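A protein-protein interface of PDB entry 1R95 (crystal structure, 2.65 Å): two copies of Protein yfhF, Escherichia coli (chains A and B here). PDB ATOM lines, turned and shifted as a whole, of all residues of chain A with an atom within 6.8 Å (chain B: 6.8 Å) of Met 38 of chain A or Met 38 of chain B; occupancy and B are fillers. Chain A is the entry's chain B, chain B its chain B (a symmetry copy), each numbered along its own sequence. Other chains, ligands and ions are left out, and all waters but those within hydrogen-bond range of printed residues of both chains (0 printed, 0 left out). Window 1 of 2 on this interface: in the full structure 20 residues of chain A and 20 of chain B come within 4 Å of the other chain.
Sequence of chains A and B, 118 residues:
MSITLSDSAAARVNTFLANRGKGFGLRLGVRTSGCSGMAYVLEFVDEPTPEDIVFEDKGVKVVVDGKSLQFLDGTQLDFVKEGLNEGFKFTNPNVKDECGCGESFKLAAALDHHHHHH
The backbone carbonyl oxygen of Met 38 of chain A sits at hydrogen-bond distance from the backbone NH of Met 38 of chain B (2.7 Å).
OH of Tyr 40 of chain B lies close to SD of Met 38 of chain A.
The backbone carbonyl oxygen of Ser 36 of chain A sits at hydrogen-bond distance from the backbone NH of Tyr 40 of chain B (3.3 Å).
The backbone carbonyl oxygen (O) of Lys 96 of chain A lies within hydrogen-bond range of the backbone NH (N) of Thr 32 of chain B, 3.3 Å away.
N of Thr 32 of chain A is in hydrogen-bond range of O of Lys 96 of chain B (3.3 Å).
The backbone NH (N) of Tyr 40 of chain A lies within hydrogen-bond range of the backbone carbonyl oxygen (O) of Ser 36 of chain B.
The side-chain sulfur (SD) of Met 38 of chain B sits close to the side-chain hydroxyl (OH) of Tyr 40 of chain A (3.7 Å).
N of Ala 39 of chain A is in hydrogen-bond range of O of Arg 31 of chain A (2.6 Å).
The backbone NH of Ala 39 of chain B is in hydrogen-bond range of the backbone carbonyl oxygen of Arg 31 of chain B, at 2.6 Å.
Lys 96 of chain B touches Arg 31 of chain A.
Thr 32 of chain A touches Val 95 of chain B.
Ser 36 of chain A touches Phe 90 of chain B.
Met 38 of chain B touches Gly 37 of chain A (O to CA, 3.3 Å).
CD1 of Tyr 40 of chain B touches N of Gly 37 of chain A, at 3.6 Å.
Val 95 of chain B touches Met 38 of chain A (CG1 to CE, 3.7 Å).
CA of Ala 39 of chain A touches O of Ser 36 of chain B, at 3.6 Å.
O of Phe 71 of chain A touches CD2 of Phe 71 of chain B, at 3.6 Å.
CB of Ser 36 of chain B touches CD1 of Phe 90 of chain A, 3.6 Å away.
Val 95 of chain A touches Val 30 of chain B.
Of chain B, only Gly 37 (3.3 Å), Met 38 (2.7 Å), Tyr 40 (3.3 Å) and Val 95 (3.7 Å) come within 4 Å of Met 38 of chain A.
Of the printed residues of chain B, Lys 96 of chain A touches Arg 31 and Thr 32.
Of the printed residues of chain A, Ser 36 of chain B touches Ala 39 (3.6 Å), Tyr 40 (3.3 Å) and Phe 90 (3.6 Å).
Printed residues of chain A within 4 Å of Met 38 of chain B: Gly 37 (3.3 Å), Met 38 (2.7 Å), Tyr 40 (3.3 Å) and Val 95 (3.7 Å).
Printed residues of chain A within 4 Å of Ala 39 of chain B: Ser 36 (3.6 Å).
Of the printed residues of chain A, Phe 71 of chain B touches Phe 71 (3.6 Å), Asn 92 (3.7 Å) and Val 95 (3.1 Å).
Printed residues of chain A within 4 Å of Asn 92 of chain B: Phe 71.
The nearest residue of chain B that does not touch Met 38 of chain A is Ser 36 of chain B (4.4 Å).
Printed residues of chain B that touch a printed residue of chain A: Val 30, Arg 31, Thr 32, Ser 36, Gly 37, Met 38, Ala 39, Tyr 40, Phe 71, Phe 90, Asn 92, Val 95 and Lys 96.
Hydrophobic or aromatic side chains of chain B within 4 Å of the printed part of chain A: Val 30, Met 38, Ala 39, Tyr 40, Phe 71, Phe 90 and Val 95.
Among the printed residues, 28 pairs touch across the chains.
Among the printed residues, no Asp or Glu carboxylate lies within 4 Å of a Lys or Arg side-chain nitrogen of the other chain.
Arg 31 of chain A touches Lys 96 of chain B, and with the chains exchanged Lys 96 of chain A touches Arg 31 of chain B.
Gly 37 of chain A touches Tyr 40 of chain B, and with the chains exchanged Tyr 40 of chain A touches Gly 37 of chain B.
Met 38 of chain A touches its own counterpart, Met 38 of chain B.
Phe 71 of chain A touches Val 95 of chain B, and with the chains exchanged Val 95 of chain A touches Phe 71 of chain B.
15 positions are printed for both chains.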
ATOM      1  N   VAL A  30     -16.927  10.557 -16.735  1.00  0.00           N
ATOM      2  CA  VAL A  30     -15.744  10.399 -15.922  1.00  0.00           C
ATOM      3  C   VAL A  30     -14.634  10.151 -16.918  1.00  0.00           C
ATOM      4  O   VAL A  30     -14.872   9.517 -17.936  1.00  0.00           O
ATOM      5  CB  VAL A  30     -15.965   9.225 -14.936  1.00  0.00           C
ATOM      6  CG1 VAL A  30     -14.798   8.261 -14.914  1.00  0.00           C
ATOM      7  CG2 VAL A  30     -16.269   9.748 -13.558  1.00  0.00           C
ATOM      8  N   ARG A  31     -13.456  10.707 -16.669  1.00  0.00           N
ATOM      9  CA  ARG A  31     -12.284  10.459 -17.511  1.00  0.00           C
ATOM     10  C   ARG A  31     -11.022  10.544 -16.651  1.00  0.00           C
ATOM     11  O   ARG A  31     -11.059  11.096 -15.546  1.00  0.00           O
ATOM     12  CB  ARG A  31     -12.223  11.442 -18.698  1.00  0.00           C
ATOM     13  CG  ARG A  31     -11.997  12.912 -18.312  1.00  0.00           C
ATOM     14  CD  ARG A  31     -11.843  13.890 -19.494  1.00  0.00           C
ATOM     15  NE  ARG A  31     -10.555  14.594 -19.449  1.00  0.00           N
ATOM     16  CZ  ARG A  31     -10.304  15.709 -18.755  1.00  0.00           C
ATOM     17  NH1 ARG A  31     -11.252  16.299 -18.031  1.00  0.00           N
ATOM     18  NH2 ARG A  31      -9.089  16.241 -18.789  1.00  0.00           N
ATOM     19  N   THR A  32      -9.909  10.006 -17.145  1.00  0.00           N
ATOM     20  CA  THR A  32      -8.653  10.103 -16.396  1.00  0.00           C
ATOM     21  C   THR A  32      -8.072  11.505 -16.504  1.00  0.00           C
ATOM     22  O   THR A  32      -8.039  12.096 -17.586  1.00  0.00           O
ATOM     23  CB  THR A  32      -7.617   9.056 -16.852  1.00  0.00           C
ATOM     24  OG1 THR A  32      -7.363   9.218 -18.252  1.00  0.00           O
ATOM     25  CG2 THR A  32      -8.184   7.639 -16.746  1.00  0.00           C
ATOM     26  N   SER A  33      -7.648  12.029 -15.357  1.00  0.00           N
ATOM     27  CA  SER A  33      -6.997  13.328 -15.262  1.00  0.00           C
ATOM     28  C   SER A  33      -5.502  13.172 -15.542  1.00  0.00           C
ATOM     29  O   SER A  33      -4.856  14.097 -16.064  1.00  0.00           O
ATOM     30  CB  SER A  33      -7.212  13.911 -13.865  1.00  0.00           C
ATOM     31  OG  SER A  33      -7.068  15.317 -13.873  1.00  0.00           O
ATOM     32  N   GLY A  34      -4.966  11.998 -15.185  1.00  0.00           N
ATOM     33  CA  GLY A  34      -3.578  11.648 -15.436  1.00  0.00           C
ATOM     34  C   GLY A  34      -2.929  10.834 -14.325  1.00  0.00           C
ATOM     35  O   GLY A  34      -2.694  11.351 -13.222  1.00  0.00           O
ATOM     36  N   SER A  36      -2.902   9.125 -11.591  1.00  0.00           N
ATOM     37  CA  SER A  36      -3.655   8.830 -10.375  1.00  0.00           C
ATOM     38  C   SER A  36      -4.760   9.883 -10.173  1.00  0.00           C
ATOM     39  O   SER A  36      -4.806  10.588  -9.159  1.00  0.00           O
ATOM     40  CB  SER A  36      -2.718   8.734  -9.165  1.00  0.00           C
ATOM     41  OG  SER A  36      -1.885   9.871  -9.061  1.00  0.00           O
ATOM     42  N   GLY A  37      -5.648   9.973 -11.159  1.00  0.00           N
ATOM     43  CA  GLY A  37      -6.648  11.023 -11.199  1.00  0.00           C
ATOM     44  C   GLY A  37      -7.869  10.740 -12.062  1.00  0.00           C
ATOM     45  O   GLY A  37      -7.771  10.139 -13.138  1.00  0.00           O
ATOM     46  N   MET A  38      -9.023  11.186 -11.568  1.00  0.00           N
ATOM     47  CA  MET A  38     -10.287  11.099 -12.284  1.00  0.00           C
ATOM     48  C   MET A  38     -10.888  12.501 -12.456  1.00  0.00           C
ATOM     49  O   MET A  38     -10.880  13.300 -11.526  1.00  0.00           O
ATOM     50  CB  MET A  38     -11.249  10.187 -11.519  1.00  0.00           C
ATOM     51  CG  MET A  38     -12.268   9.445 -12.397  1.00  0.00           C
ATOM     52  SD  MET A  38     -12.091   7.626 -12.355  1.00  0.00           S
ATOM     53  CE  MET A  38     -10.461   7.400 -13.153  1.00  0.00           C
ATOM     54  N   ALA A  39     -11.384  12.808 -13.648  1.00  0.00           N
ATOM     55  CA  ALA A  39     -12.139  14.047 -13.853  1.00  0.00           C
ATOM     56  C   ALA A  39     -13.590  13.800 -14.293  1.00  0.00           C
ATOM     57  O   ALA A  39     -13.860  13.020 -15.205  1.00  0.00           O
ATOM     58  CB  ALA A  39     -11.427  14.982 -14.828  1.00  0.00           C
ATOM     59  N   TYR A  40     -14.506  14.477 -13.609  1.00  0.00           N
ATOM     60  CA  TYR A  40     -15.920  14.487 -13.953  1.00  0.00           C
ATOM     61  C   TYR A  40     -16.178  15.272 -15.233  1.00  0.00           C
ATOM     62  O   TYR A  40     -15.586  16.309 -15.461  1.00  0.00           O
ATOM     63  CB  TYR A  40     -16.683  15.153 -12.835  1.00  0.00           C
ATOM     64  CG  TYR A  40     -16.699  14.384 -11.547  1.00  0.00           C
ATOM     65  CD1 TYR A  40     -16.126  14.909 -10.395  1.00  0.00           C
ATOM     66  CD2 TYR A  40     -17.311  13.138 -11.469  1.00  0.00           C
ATOM     67  CE1 TYR A  40     -16.151  14.202  -9.193  1.00  0.00           C
ATOM     68  CE2 TYR A  40     -17.348  12.434 -10.276  1.00  0.00           C
ATOM     69  CZ  TYR A  40     -16.768  12.971  -9.146  1.00  0.00           C
ATOM     70  OH  TYR A  40     -16.815  12.257  -7.976  1.00  0.00           O
ATOM     71  N   PHE A  71     -18.535   4.939 -10.287  1.00  0.00           N
ATOM     72  CA  PHE A  71     -17.864   6.184  -9.896  1.00  0.00           C
ATOM     73  C   PHE A  71     -18.829   7.329  -9.546  1.00  0.00           C
ATOM     74  O   PHE A  71     -18.535   8.130  -8.658  1.00  0.00           O
ATOM     75  CB  PHE A  71     -16.842   6.650 -10.950  1.00  0.00           C
ATOM     76  CG  PHE A  71     -16.131   5.521 -11.660  1.00  0.00           C
ATOM     77  CD1 PHE A  71     -16.562   5.087 -12.920  1.00  0.00           C
ATOM     78  CD2 PHE A  71     -15.026   4.890 -11.075  1.00  0.00           C
ATOM     79  CE1 PHE A  71     -15.920   4.040 -13.585  1.00  0.00           C
ATOM     80  CE2 PHE A  71     -14.371   3.839 -11.736  1.00  0.00           C
ATOM     81  CZ  PHE A  71     -14.821   3.410 -12.991  1.00  0.00           C
ATOM     82  N   PHE A  90     -19.041  19.034  -8.133  1.00  0.00           N
ATOM     83  CA  PHE A  90     -19.483  17.681  -7.808  1.00  0.00           C
ATOM     84  C   PHE A  90     -19.143  17.348  -6.372  1.00  0.00           C
ATOM     85  O   PHE A  90     -18.040  17.587  -5.916  1.00  0.00           O
ATOM     86  CB  PHE A  90     -18.808  16.680  -8.727  1.00  0.00           C
ATOM     87  CG  PHE A  90     -19.110  16.881 -10.174  1.00  0.00           C
ATOM     88  CD1 PHE A  90     -18.567  17.958 -10.870  1.00  0.00           C
ATOM     89  CD2 PHE A  90     -19.928  15.983 -10.855  1.00  0.00           C
ATOM     90  CE1 PHE A  90     -18.834  18.148 -12.232  1.00  0.00           C
ATOM     91  CE2 PHE A  90     -20.205  16.163 -12.212  1.00  0.00           C
ATOM     92  CZ  PHE A  90     -19.649  17.256 -12.902  1.00  0.00           C
ATOM     93  N   ASN A  92     -19.596  14.364  -3.095  1.00  0.00           N
ATOM     94  CA  ASN A  92     -19.983  13.061  -2.584  1.00  0.00           C
ATOM     95  C   ASN A  92     -19.834  13.081  -1.063  1.00  0.00           C
ATOM     96  O   ASN A  92     -18.811  13.549  -0.538  1.00  0.00           O
ATOM     97  CB  ASN A  92     -19.124  11.952  -3.193  1.00  0.00           C
ATOM     98  CG  ASN A  92     -19.919  10.707  -3.510  1.00  0.00           C
ATOM     99  OD1 ASN A  92     -20.564  10.130  -2.635  1.00  0.00           O
ATOM    100  ND2 ASN A  92     -19.876  10.282  -4.769  1.00  0.00           N
ATOM    101  N   VAL A  95     -17.003  10.391  -0.387  1.00  0.00           N
ATOM    102  CA  VAL A  95     -15.662  10.942  -0.611  1.00  0.00           C
ATOM    103  C   VAL A  95     -15.420  12.106   0.353  1.00  0.00           C
ATOM    104  O   VAL A  95     -16.352  12.565   1.017  1.00  0.00           O
ATOM    105  CB  VAL A  95     -15.473  11.407  -2.081  1.00  0.00           C
ATOM    106  CG1 VAL A  95     -14.147  12.109  -2.281  1.00  0.00           C
ATOM    107  CG2 VAL A  95     -15.544  10.243  -3.014  1.00  0.00           C
ATOM    108  N   LYS A  96     -14.173  12.567   0.441  1.00  0.00           N
ATOM    109  CA  LYS A  96     -13.814  13.674   1.324  1.00  0.00           C
ATOM    110  C   LYS A  96     -12.608  14.473   0.815  1.00  0.00           C
ATOM    111  O   LYS A  96     -11.986  14.109  -0.196  1.00  0.00           O
ATOM    112  CB  LYS A  96     -13.566  13.166   2.754  1.00  0.00           C
ATOM    113  N   VAL B  30      -9.051   7.644  -2.011  1.00  0.00           N
ATOM    114  CA  VAL B  30      -9.623   8.517  -3.010  1.00  0.00           C
ATOM    115  C   VAL B  30      -9.818   9.832  -2.291  1.00  0.00           C
ATOM    116  O   VAL B  30     -10.125   9.829  -1.108  1.00  0.00           O
ATOM    117  CB  VAL B  30     -10.941   7.891  -3.528  1.00  0.00           C
ATOM    118  CG1 VAL B  30     -12.080   8.888  -3.558  1.00  0.00           C
ATOM    119  CG2 VAL B  30     -10.728   7.262  -4.878  1.00  0.00           C
ATOM    120  N   ARG B  31      -9.570  10.942  -2.973  1.00  0.00           N
ATOM    121  CA  ARG B  31      -9.816  12.272  -2.413  1.00  0.00           C
ATOM    122  C   ARG B  31     -10.182  13.234  -3.544  1.00  0.00           C
ATOM    123  O   ARG B  31      -9.924  12.941  -4.718  1.00  0.00           O
ATOM    124  CB  ARG B  31      -8.598  12.782  -1.614  1.00  0.00           C
ATOM    125  CG  ARG B  31      -7.339  13.048  -2.452  1.00  0.00           C
ATOM    126  CD  ARG B  31      -6.145  13.645  -1.679  1.00  0.00           C
ATOM    127  NE  ARG B  31      -5.726  14.934  -2.242  1.00  0.00           N
ATOM    128  CZ  ARG B  31      -4.884  15.096  -3.268  1.00  0.00           C
ATOM    129  NH1 ARG B  31      -4.326  14.051  -3.874  1.00  0.00           N
ATOM    130  NH2 ARG B  31      -4.596  16.321  -3.691  1.00  0.00           N
ATOM    131  N   THR B  32     -10.779  14.375  -3.208  1.00  0.00           N
ATOM    132  CA  THR B  32     -11.106  15.364  -4.239  1.00  0.00           C
ATOM    133  C   THR B  32      -9.854  16.102  -4.688  1.00  0.00           C
ATOM    134  O   THR B  32      -9.030  16.512  -3.866  1.00  0.00           O
ATOM    135  CB  THR B  32     -12.181  16.364  -3.771  1.00  0.00           C
ATOM    136  OG1 THR B  32     -11.728  17.028  -2.586  1.00  0.00           O
ATOM    137  CG2 THR B  32     -13.449  15.637  -3.319  1.00  0.00           C
ATOM    138  N   SER B  33      -9.718  16.232  -6.004  1.00  0.00           N
ATOM    139  CA  SER B  33      -8.628  16.968  -6.629  1.00  0.00           C
ATOM    140  C   SER B  33      -8.985  18.454  -6.695  1.00  0.00           C
ATOM    141  O   SER B  33      -8.095  19.321  -6.639  1.00  0.00           O
ATOM    142  CB  SER B  33      -8.378  16.425  -8.036  1.00  0.00           C
ATOM    143  OG  SER B  33      -7.066  16.720  -8.471  1.00  0.00           O
ATOM    144  N   GLY B  34     -10.288  18.730  -6.818  1.00  0.00           N
ATOM    145  CA  GLY B  34     -10.818  20.083  -6.828  1.00  0.00           C
ATOM    146  C   GLY B  34     -11.988  20.289  -7.781  1.00  0.00           C
ATOM    147  O   GLY B  34     -11.812  20.252  -9.009  1.00  0.00           O
ATOM    148  N   SER B  36     -14.293  19.335  -9.823  1.00  0.00           N
ATOM    149  CA  SER B  36     -14.734  18.236 -10.676  1.00  0.00           C
ATOM    150  C   SER B  36     -13.578  17.244 -10.893  1.00  0.00           C
ATOM    151  O   SER B  36     -13.149  16.985 -12.024  1.00  0.00           O
ATOM    152  CB  SER B  36     -15.299  18.767 -11.999  1.00  0.00           C
ATOM    153  OG  SER B  36     -14.398  19.655 -12.629  1.00  0.00           O
ATOM    154  N   GLY B  37     -13.083  16.694  -9.788  1.00  0.00           N
ATOM    155  CA  GLY B  37     -11.889  15.870  -9.807  1.00  0.00           C
ATOM    156  C   GLY B  37     -11.717  14.928  -8.626  1.00  0.00           C
ATOM    157  O   GLY B  37     -12.041  15.265  -7.481  1.00  0.00           O
ATOM    158  N   MET B  38     -11.200  13.737  -8.926  1.00  0.00           N
ATOM    159  CA  MET B  38     -10.871  12.732  -7.926  1.00  0.00           C
ATOM    160  C   MET B  38      -9.384  12.366  -8.023  1.00  0.00           C
ATOM    161  O   MET B  38      -8.856  12.194  -9.116  1.00  0.00           O
ATOM    162  CB  MET B  38     -11.749  11.495  -8.132  1.00  0.00           C
ATOM    163  CG  MET B  38     -12.047  10.698  -6.854  1.00  0.00           C
ATOM    164  SD  MET B  38     -13.820  10.652  -6.411  1.00  0.00           S
ATOM    165  CE  MET B  38     -14.141  12.408  -6.010  1.00  0.00           C
ATOM    166  N   ALA B  39      -8.705  12.273  -6.886  1.00  0.00           N
ATOM    167  CA  ALA B  39      -7.336  11.751  -6.868  1.00  0.00           C
ATOM    168  C   ALA B  39      -7.192  10.471  -6.031  1.00  0.00           C
ATOM    169  O   ALA B  39      -7.658  10.391  -4.896  1.00  0.00           O
ATOM    170  CB  ALA B  39      -6.337  12.814  -6.413  1.00  0.00           C
ATOM    171  N   TYR B  40      -6.546   9.478  -6.633  1.00  0.00           N
ATOM    172  CA  TYR B  40      -6.189   8.234  -5.968  1.00  0.00           C
ATOM    173  C   TYR B  40      -5.078   8.445  -4.947  1.00  0.00           C
ATOM    174  O   TYR B  40      -4.145   9.188  -5.182  1.00  0.00           O
ATOM    175  CB  TYR B  40      -5.690   7.259  -7.006  1.00  0.00           C
ATOM    176  CG  TYR B  40      -6.737   6.787  -7.971  1.00  0.00           C
ATOM    177  CD1 TYR B  40      -6.629   7.056  -9.330  1.00  0.00           C
ATOM    178  CD2 TYR B  40      -7.827   6.044  -7.532  1.00  0.00           C
ATOM    179  CE1 TYR B  40      -7.594   6.607 -10.231  1.00  0.00           C
ATOM    180  CE2 TYR B  40      -8.785   5.586  -8.422  1.00  0.00           C
ATOM    181  CZ  TYR B  40      -8.662   5.870  -9.766  1.00  0.00           C
ATOM    182  OH  TYR B  40      -9.621   5.408 -10.630  1.00  0.00           O
ATOM    183  N   PHE B  71     -15.689   3.629  -5.954  1.00  0.00           N
ATOM    184  CA  PHE B  71     -14.726   4.292  -6.841  1.00  0.00           C
ATOM    185  C   PHE B  71     -13.545   3.401  -7.257  1.00  0.00           C
ATOM    186  O   PHE B  71     -13.056   3.512  -8.382  1.00  0.00           O
ATOM    187  CB  PHE B  71     -14.212   5.620  -6.254  1.00  0.00           C
ATOM    188  CG  PHE B  71     -15.242   6.376  -5.447  1.00  0.00           C
ATOM    189  CD1 PHE B  71     -15.264   6.282  -4.049  1.00  0.00           C
ATOM    190  CD2 PHE B  71     -16.193   7.188  -6.079  1.00  0.00           C
ATOM    191  CE1 PHE B  71     -16.214   6.969  -3.291  1.00  0.00           C
ATOM    192  CE2 PHE B  71     -17.151   7.885  -5.326  1.00  0.00           C
ATOM    193  CZ  PHE B  71     -17.165   7.772  -3.930  1.00  0.00           C
ATOM    194  N   PHE B  90      -2.723   4.089 -11.892  1.00  0.00           N
ATOM    195  CA  PHE B  90      -4.009   3.424 -11.693  1.00  0.00           C
ATOM    196  C   PHE B  90      -4.743   3.296 -13.009  1.00  0.00           C
ATOM    197  O   PHE B  90      -4.834   4.240 -13.772  1.00  0.00           O
ATOM    198  CB  PHE B  90      -4.859   4.221 -10.721  1.00  0.00           C
ATOM    199  CG  PHE B  90      -4.253   4.374  -9.367  1.00  0.00           C
ATOM    200  CD1 PHE B  90      -3.158   5.211  -9.168  1.00  0.00           C
ATOM    201  CD2 PHE B  90      -4.787   3.694  -8.275  1.00  0.00           C
ATOM    202  CE1 PHE B  90      -2.591   5.371  -7.897  1.00  0.00           C
ATOM    203  CE2 PHE B  90      -4.229   3.842  -7.002  1.00  0.00           C
ATOM    204  CZ  PHE B  90      -3.122   4.691  -6.818  1.00  0.00           C
ATOM    205  N   ASN B  92      -8.307   1.588 -15.066  1.00  0.00           N
ATOM    206  CA  ASN B  92      -9.601   0.928 -15.067  1.00  0.00           C
ATOM    207  C   ASN B  92      -9.986   0.633 -16.516  1.00  0.00           C
ATOM    208  O   ASN B  92      -9.860   1.505 -17.390  1.00  0.00           O
ATOM    209  CB  ASN B  92     -10.664   1.798 -14.395  1.00  0.00           C
ATOM    210  CG  ASN B  92     -11.622   0.995 -13.547  1.00  0.00           C
ATOM    211  OD1 ASN B  92     -12.267   0.065 -14.029  1.00  0.00           O
ATOM    212  ND2 ASN B  92     -11.723   1.352 -12.269  1.00  0.00           N
ATOM    213  N   VAL B  95     -13.237   2.831 -17.064  1.00  0.00           N
ATOM    214  CA  VAL B  95     -12.907   4.232 -17.348  1.00  0.00           C
ATOM    215  C   VAL B  95     -12.083   4.312 -18.635  1.00  0.00           C
ATOM    216  O   VAL B  95     -11.638   3.286 -19.152  1.00  0.00           O
ATOM    217  CB  VAL B  95     -12.136   4.887 -16.169  1.00  0.00           C
ATOM    218  CG1 VAL B  95     -11.666   6.284 -16.515  1.00  0.00           C
ATOM    219  CG2 VAL B  95     -12.999   4.961 -14.952  1.00  0.00           C
ATOM    220  N   LYS B  96     -11.899   5.524 -19.158  1.00  0.00           N
ATOM    221  CA  LYS B  96     -11.131   5.733 -20.383  1.00  0.00           C
ATOM    222  C   LYS B  96     -10.470   7.115 -20.441  1.00  0.00           C
ATOM    223  O   LYS B  96     -10.681   7.958 -19.556  1.00  0.00           O
ATOM    224  CB  LYS B  96     -12.014   5.499 -21.620  1.00  0.00           C
